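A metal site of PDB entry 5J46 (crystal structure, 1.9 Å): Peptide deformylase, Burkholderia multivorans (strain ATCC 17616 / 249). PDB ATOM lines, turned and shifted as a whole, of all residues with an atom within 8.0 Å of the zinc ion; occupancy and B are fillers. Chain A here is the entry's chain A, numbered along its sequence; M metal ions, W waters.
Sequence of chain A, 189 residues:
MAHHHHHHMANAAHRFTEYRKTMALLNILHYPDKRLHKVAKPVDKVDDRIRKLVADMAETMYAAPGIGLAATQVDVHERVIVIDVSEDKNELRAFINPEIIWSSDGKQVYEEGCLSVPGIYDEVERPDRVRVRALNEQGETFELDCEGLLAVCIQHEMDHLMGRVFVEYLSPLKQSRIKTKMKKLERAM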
ATOM      1  N   ILE A  28      17.378  20.910  30.025  1.00  0.00           N
ATOM      2  CA  ILE A  28      17.642  21.165  28.609  1.00  0.00           C
ATOM      3  C   ILE A  28      16.991  22.501  28.222  1.00  0.00           C
ATOM      4  O   ILE A  28      15.769  22.664  28.362  1.00  0.00           O
ATOM      5  CB  ILE A  28      17.134  20.019  27.719  1.00  0.00           C
ATOM      6  CG1 ILE A  28      17.844  18.708  28.077  1.00  0.00           C
ATOM      7  CG2 ILE A  28      17.355  20.355  26.214  1.00  0.00           C
ATOM      8  CD1 ILE A  28      17.386  17.465  27.303  1.00  0.00           C
ATOM      9  N   LEU A  36      21.443  29.223  23.920  1.00  0.00           N
ATOM     10  CA  LEU A  36      21.712  28.229  22.888  1.00  0.00           C
ATOM     11  C   LEU A  36      22.552  28.770  21.737  1.00  0.00           C
ATOM     12  O   LEU A  36      22.926  27.989  20.850  1.00  0.00           O
ATOM     13  CB  LEU A  36      20.402  27.665  22.343  1.00  0.00           C
ATOM     14  CG  LEU A  36      19.644  26.738  23.291  1.00  0.00           C
ATOM     15  CD1 LEU A  36      18.261  26.445  22.711  1.00  0.00           C
ATOM     16  CD2 LEU A  36      20.462  25.471  23.480  1.00  0.00           C
ATOM     17  N   GLY A  68      20.945  12.256  20.855  1.00  0.00           N
ATOM     18  CA  GLY A  68      22.192  12.997  21.005  1.00  0.00           C
ATOM     19  C   GLY A  68      21.963  14.202  21.880  1.00  0.00           C
ATOM     20  O   GLY A  68      20.823  14.575  22.166  1.00  0.00           O
ATOM     21  N   LEU A  69      23.068  14.812  22.317  1.00  0.00           N
ATOM     22  CA  LEU A  69      22.991  15.984  23.182  1.00  0.00           C
ATOM     23  C   LEU A  69      24.340  16.707  23.165  1.00  0.00           C
ATOM     24  O   LEU A  69      25.382  16.058  23.184  1.00  0.00           O
ATOM     25  CB  LEU A  69      22.623  15.578  24.616  1.00  0.00           C
ATOM     26  CG  LEU A  69      22.259  16.686  25.607  1.00  0.00           C
ATOM     27  CD1 LEU A  69      20.937  17.358  25.215  1.00  0.00           C
ATOM     28  CD2 LEU A  69      22.160  16.177  27.068  1.00  0.00           C
ATOM     29  N   ALA A  70      24.304  18.039  23.094  1.00  0.00           N
ATOM     30  CA  ALA A  70      25.513  18.863  23.188  1.00  0.00           C
ATOM     31  C   ALA A  70      25.501  19.589  24.524  1.00  0.00           C
ATOM     32  O   ALA A  70      24.436  19.968  25.024  1.00  0.00           O
ATOM     33  CB  ALA A  70      25.596  19.880  22.045  1.00  0.00           C
ATOM     34  N   GLN A  73      23.393  22.634  25.233  1.00  0.00           N
ATOM     35  CA  GLN A  73      21.963  22.508  25.482  1.00  0.00           C
ATOM     36  C   GLN A  73      21.617  22.426  26.955  1.00  0.00           C
ATOM     37  O   GLN A  73      20.453  22.665  27.310  1.00  0.00           O
ATOM     38  CB  GLN A  73      21.415  21.273  24.760  1.00  0.00           C
ATOM     39  CG  GLN A  73      21.611  21.317  23.249  1.00  0.00           C
ATOM     40  CD  GLN A  73      21.022  20.122  22.557  1.00  0.00           C
ATOM     41  OE1 GLN A  73      21.750  19.228  22.101  1.00  0.00           O
ATOM     42  NE2 GLN A  73      19.678  20.093  22.462  1.00  0.00           N
ATOM     43  N   GLU A 112      14.876  16.405  10.796  1.00  0.00           N
ATOM     44  CA  GLU A 112      15.454  16.449  12.132  1.00  0.00           C
ATOM     45  C   GLU A 112      14.441  16.975  13.133  1.00  0.00           C
ATOM     46  O   GLU A 112      13.617  17.830  12.809  1.00  0.00           O
ATOM     47  CB  GLU A 112      16.710  17.330  12.187  1.00  0.00           C
ATOM     48  CG  GLU A 112      17.777  16.852  11.223  1.00  0.00           C
ATOM     49  CD  GLU A 112      19.052  17.676  11.221  1.00  0.00           C
ATOM     50  OE1 GLU A 112      19.319  18.422  12.193  1.00  0.00           O
ATOM     51  OE2 GLU A 112      19.819  17.534  10.235  1.00  0.00           O
ATOM     52  N   GLY A 113      14.491  16.421  14.349  1.00  0.00           N
ATOM     53  CA  GLY A 113      13.959  17.058  15.530  1.00  0.00           C
ATOM     54  C   GLY A 113      15.112  17.448  16.446  1.00  0.00           C
ATOM     55  O   GLY A 113      16.283  17.233  16.161  1.00  0.00           O
ATOM     56  N   CYS A 114      14.743  18.030  17.583  1.00  0.00           N
ATOM     57  CA  CYS A 114      15.781  18.550  18.471  1.00  0.00           C
ATOM     58  C   CYS A 114      15.214  18.584  19.882  1.00  0.00           C
ATOM     59  O   CYS A 114      14.101  19.063  20.091  1.00  0.00           O
ATOM     60  CB  CYS A 114      16.244  19.946  18.037  1.00  0.00           C
ATOM     61  SG  CYS A 114      17.551  20.664  19.115  1.00  0.00           S
ATOM     62  N   LEU A 115      16.007  18.096  20.830  1.00  0.00           N
ATOM     63  CA  LEU A 115      15.584  18.129  22.228  1.00  0.00           C
ATOM     64  C   LEU A 115      15.418  19.555  22.750  1.00  0.00           C
ATOM     65  O   LEU A 115      14.704  19.746  23.727  1.00  0.00           O
ATOM     66  CB  LEU A 115      16.604  17.340  23.072  1.00  0.00           C
ATOM     67  CG  LEU A 115      16.628  15.825  22.835  1.00  0.00           C
ATOM     68  CD1 LEU A 115      17.736  15.131  23.670  1.00  0.00           C
ATOM     69  CD2 LEU A 115      15.279  15.186  23.135  1.00  0.00           C
ATOM     70  N   SER A 116      16.016  20.563  22.107  1.00  0.00           N
ATOM     71  CA  SER A 116      15.797  21.957  22.489  1.00  0.00           C
ATOM     72  C   SER A 116      14.640  22.622  21.746  1.00  0.00           C
ATOM     73  O   SER A 116      14.417  23.820  21.918  1.00  0.00           O
ATOM     74  CB  SER A 116      17.072  22.786  22.267  1.00  0.00           C
ATOM     75  OG  SER A 116      18.045  22.471  23.263  1.00  0.00           O
ATOM     76  N   VAL A 117      13.924  21.891  20.891  1.00  0.00           N
ATOM     77  CA  VAL A 117      12.816  22.444  20.122  1.00  0.00           C
ATOM     78  C   VAL A 117      11.685  21.425  20.133  1.00  0.00           C
ATOM     79  O   VAL A 117      11.385  20.841  19.082  1.00  0.00           O
ATOM     80  CB  VAL A 117      13.234  22.765  18.678  1.00  0.00           C
ATOM     81  CG1 VAL A 117      12.276  23.751  18.024  1.00  0.00           C
ATOM     82  CG2 VAL A 117      14.676  23.291  18.616  1.00  0.00           C
ATOM     83  N   ARG A 126      22.529  18.434   4.660  1.00  0.00           N
ATOM     84  CA  ARG A 126      23.869  18.375   5.219  1.00  0.00           C
ATOM     85  C   ARG A 126      24.737  17.489   4.347  1.00  0.00           C
ATOM     86  O   ARG A 126      24.217  16.672   3.585  1.00  0.00           O
ATOM     87  CB  ARG A 126      23.869  17.823   6.650  1.00  0.00           C
ATOM     88  CG  ARG A 126      22.985  18.563   7.643  1.00  0.00           C
ATOM     89  CD  ARG A 126      23.227  18.011   9.053  1.00  0.00           C
ATOM     90  NE  ARG A 126      22.304  18.537  10.050  1.00  0.00           N
ATOM     91  CZ  ARG A 126      22.541  19.620  10.790  1.00  0.00           C
ATOM     92  NH1 ARG A 126      23.676  20.303  10.630  1.00  0.00           N
ATOM     93  NH2 ARG A 126      21.644  20.019  11.689  1.00  0.00           N
ATOM     94  N   CYS A 153      23.584  13.149  12.919  1.00  0.00           N
ATOM     95  CA  CYS A 153      23.550  13.487  14.344  1.00  0.00           C
ATOM     96  C   CYS A 153      24.809  14.243  14.768  1.00  0.00           C
ATOM     97  O   CYS A 153      24.715  15.226  15.513  1.00  0.00           O
ATOM     98  CB  CYS A 153      23.386  12.211  15.167  1.00  0.00           C
ATOM     99  SG  CYS A 153      22.970  12.516  16.883  1.00  0.00           S
ATOM    100  N   HIS A 156      24.592  17.759  13.545  1.00  0.00           N
ATOM    101  CA  HIS A 156      23.590  18.435  14.371  1.00  0.00           C
ATOM    102  C   HIS A 156      24.159  18.804  15.729  1.00  0.00           C
ATOM    103  O   HIS A 156      24.006  19.947  16.188  1.00  0.00           O
ATOM    104  CB  HIS A 156      22.378  17.519  14.517  1.00  0.00           C
ATOM    105  CG  HIS A 156      21.273  18.071  15.377  1.00  0.00           C
ATOM    106  ND1 HIS A 156      20.056  18.475  14.862  1.00  0.00           N
ATOM    107  CD2 HIS A 156      21.195  18.270  16.718  1.00  0.00           C
ATOM    108  CE1 HIS A 156      19.280  18.895  15.849  1.00  0.00           C
ATOM    109  NE2 HIS A 156      19.945  18.781  16.988  1.00  0.00           N
ATOM    110  N   GLU A 157      24.824  17.861  16.416  1.00  0.00           N
ATOM    111  CA  GLU A 157      25.318  18.174  17.759  1.00  0.00           C
ATOM    112  C   GLU A 157      26.488  19.158  17.696  1.00  0.00           C
ATOM    113  O   GLU A 157      26.592  20.040  18.553  1.00  0.00           O
ATOM    114  CB  GLU A 157      25.760  16.909  18.510  1.00  0.00           C
ATOM    115  CG  GLU A 157      24.765  15.743  18.626  1.00  0.00           C
ATOM    116  CD  GLU A 157      23.335  16.143  19.010  1.00  0.00           C
ATOM    117  OE1 GLU A 157      22.425  15.349  18.684  1.00  0.00           O
ATOM    118  OE2 GLU A 157      23.132  17.204  19.646  1.00  0.00           O
ATOM    119  N   ASP A 159      26.882  21.490  15.478  1.00  0.00           N
ATOM    120  CA  ASP A 159      26.245  22.781  15.273  1.00  0.00           C
ATOM    121  C   ASP A 159      25.870  23.413  16.621  1.00  0.00           C
ATOM    122  O   ASP A 159      26.061  24.619  16.817  1.00  0.00           O
ATOM    123  CB  ASP A 159      24.985  22.629  14.395  1.00  0.00           C
ATOM    124  CG  ASP A 159      25.256  22.819  12.916  1.00  0.00           C
ATOM    125  OD1 ASP A 159      26.405  23.058  12.510  1.00  0.00           O
ATOM    126  OD2 ASP A 159      24.277  22.705  12.130  1.00  0.00           O
ATOM    127  N   HIS A 160      25.334  22.619  17.551  1.00  0.00           N
ATOM    128  CA  HIS A 160      24.933  23.157  18.849  1.00  0.00           C
ATOM    129  C   HIS A 160      26.098  23.837  19.568  1.00  0.00           C
ATOM    130  O   HIS A 160      25.919  24.881  20.198  1.00  0.00           O
ATOM    131  CB  HIS A 160      24.364  22.055  19.749  1.00  0.00           C
ATOM    132  CG  HIS A 160      22.899  21.766  19.566  1.00  0.00           C
ATOM    133  ND1 HIS A 160      21.922  22.712  19.789  1.00  0.00           N
ATOM    134  CD2 HIS A 160      22.254  20.622  19.255  1.00  0.00           C
ATOM    135  CE1 HIS A 160      20.738  22.168  19.585  1.00  0.00           C
ATOM    136  NE2 HIS A 160      20.903  20.897  19.268  1.00  0.00           N
ATOM    137  N   ARG A 164      24.415  27.019  17.117  1.00  0.00           N
ATOM    138  CA  ARG A 164      23.477  26.890  16.003  1.00  0.00           C
ATOM    139  C   ARG A 164      22.399  25.854  16.307  1.00  0.00           C
ATOM    140  O   ARG A 164      22.724  24.709  16.624  1.00  0.00           O
ATOM    141  CB  ARG A 164      24.189  26.509  14.711  1.00  0.00           C
ATOM    142  CG  ARG A 164      23.375  26.691  13.448  1.00  0.00           C
ATOM    143  CD  ARG A 164      24.265  26.610  12.195  1.00  0.00           C
ATOM    144  NE  ARG A 164      25.242  27.702  12.076  1.00  0.00           N
ATOM    145  CZ  ARG A 164      26.550  27.607  12.354  1.00  0.00           C
ATOM    146  NH1 ARG A 164      27.062  26.463  12.787  1.00  0.00           N
ATOM    147  NH2 ARG A 164      27.336  28.665  12.208  1.00  0.00           N
ATOM    148  N   VAL A 165      21.126  26.258  16.174  1.00  0.00           N
ATOM    149  CA  VAL A 165      19.974  25.361  16.267  1.00  0.00           C
ATOM    150  C   VAL A 165      19.457  25.118  14.846  1.00  0.00           C
ATOM    151  O   VAL A 165      19.543  25.993  13.976  1.00  0.00           O
ATOM    152  CB  VAL A 165      18.870  25.955  17.169  1.00  0.00           C
ATOM    153  CG1 VAL A 165      17.692  24.976  17.331  1.00  0.00           C
ATOM    154  CG2 VAL A 165      19.458  26.384  18.504  1.00  0.00           C
ATOM    155  N   PHE A 166      18.927  23.919  14.599  1.00  0.00           N
ATOM    156  CA  PHE A 166      18.683  23.497  13.222  1.00  0.00           C
ATOM    157  C   PHE A 166      17.619  24.353  12.545  1.00  0.00           C
ATOM    158  O   PHE A 166      17.616  24.491  11.315  1.00  0.00           O
ATOM    159  CB  PHE A 166      18.307  22.009  13.158  1.00  0.00           C
ATOM    160  CG  PHE A 166      16.840  21.730  13.420  1.00  0.00           C
ATOM    161  CD1 PHE A 166      16.359  21.619  14.708  1.00  0.00           C
ATOM    162  CD2 PHE A 166      15.962  21.553  12.356  1.00  0.00           C
ATOM    163  CE1 PHE A 166      15.004  21.348  14.944  1.00  0.00           C
ATOM    164  CE2 PHE A 166      14.614  21.295  12.591  1.00  0.00           C
ATOM    165  CZ  PHE A 166      14.147  21.184  13.882  1.00  0.00           C
HETATM  166 ZN    ZN M   1      19.490  19.420  18.965  1.00  0.00          ZN
HETATM  167  O   HOH W   1      19.305  22.104  16.748  1.00  0.00           O
HETATM  168  O   HOH W   2      20.221  18.171  20.547  1.00  0.00           O
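The zinc ion is bound by a ring nitrogen (NE2) of His 160 (2.1 Å), a ring nitrogen (NE2) of His 156 (2.1 Å), water W2 (2.1 Å) and the side-chain sulfur of Cys 114 (2.3 Å). The zinc ion has four donor atoms within binding distance.
The side-chain amide oxygen of Gln 73 lies close to a ring nitrogen (NE2) of His 160, 3.4 Å away. The side-chain carboxylate (OE1) of Glu 112 sits at hydrogen-bond distance from a ring nitrogen (ND1) of His 156, at 2.8 Å. SG of Cys 114 sits close to N of Ser 116, at 3.4 Å. OE2 of Glu 157 sits close to OE1 of Gln 73 (3.5 Å). The side-chain hydroxyl (OG) of Ser 116 lies within hydrogen-bond range of the side-chain amide nitrogen (NE2) of Gln 73 (3.0 Å). OE1 of Gln 73 is in hydrogen-bond range of N of Ala 70.
Water W2 bridges the side-chain amide oxygen (OE1) of Gln 73 and the side-chain carboxylate (OE2) of Glu 157.
Gln 73 touches the zinc ion (NE2 to ZN, 3.6 Å). Within 4 Å of the zinc ion: Gln 73, Cys 114, His 156 and His 160.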
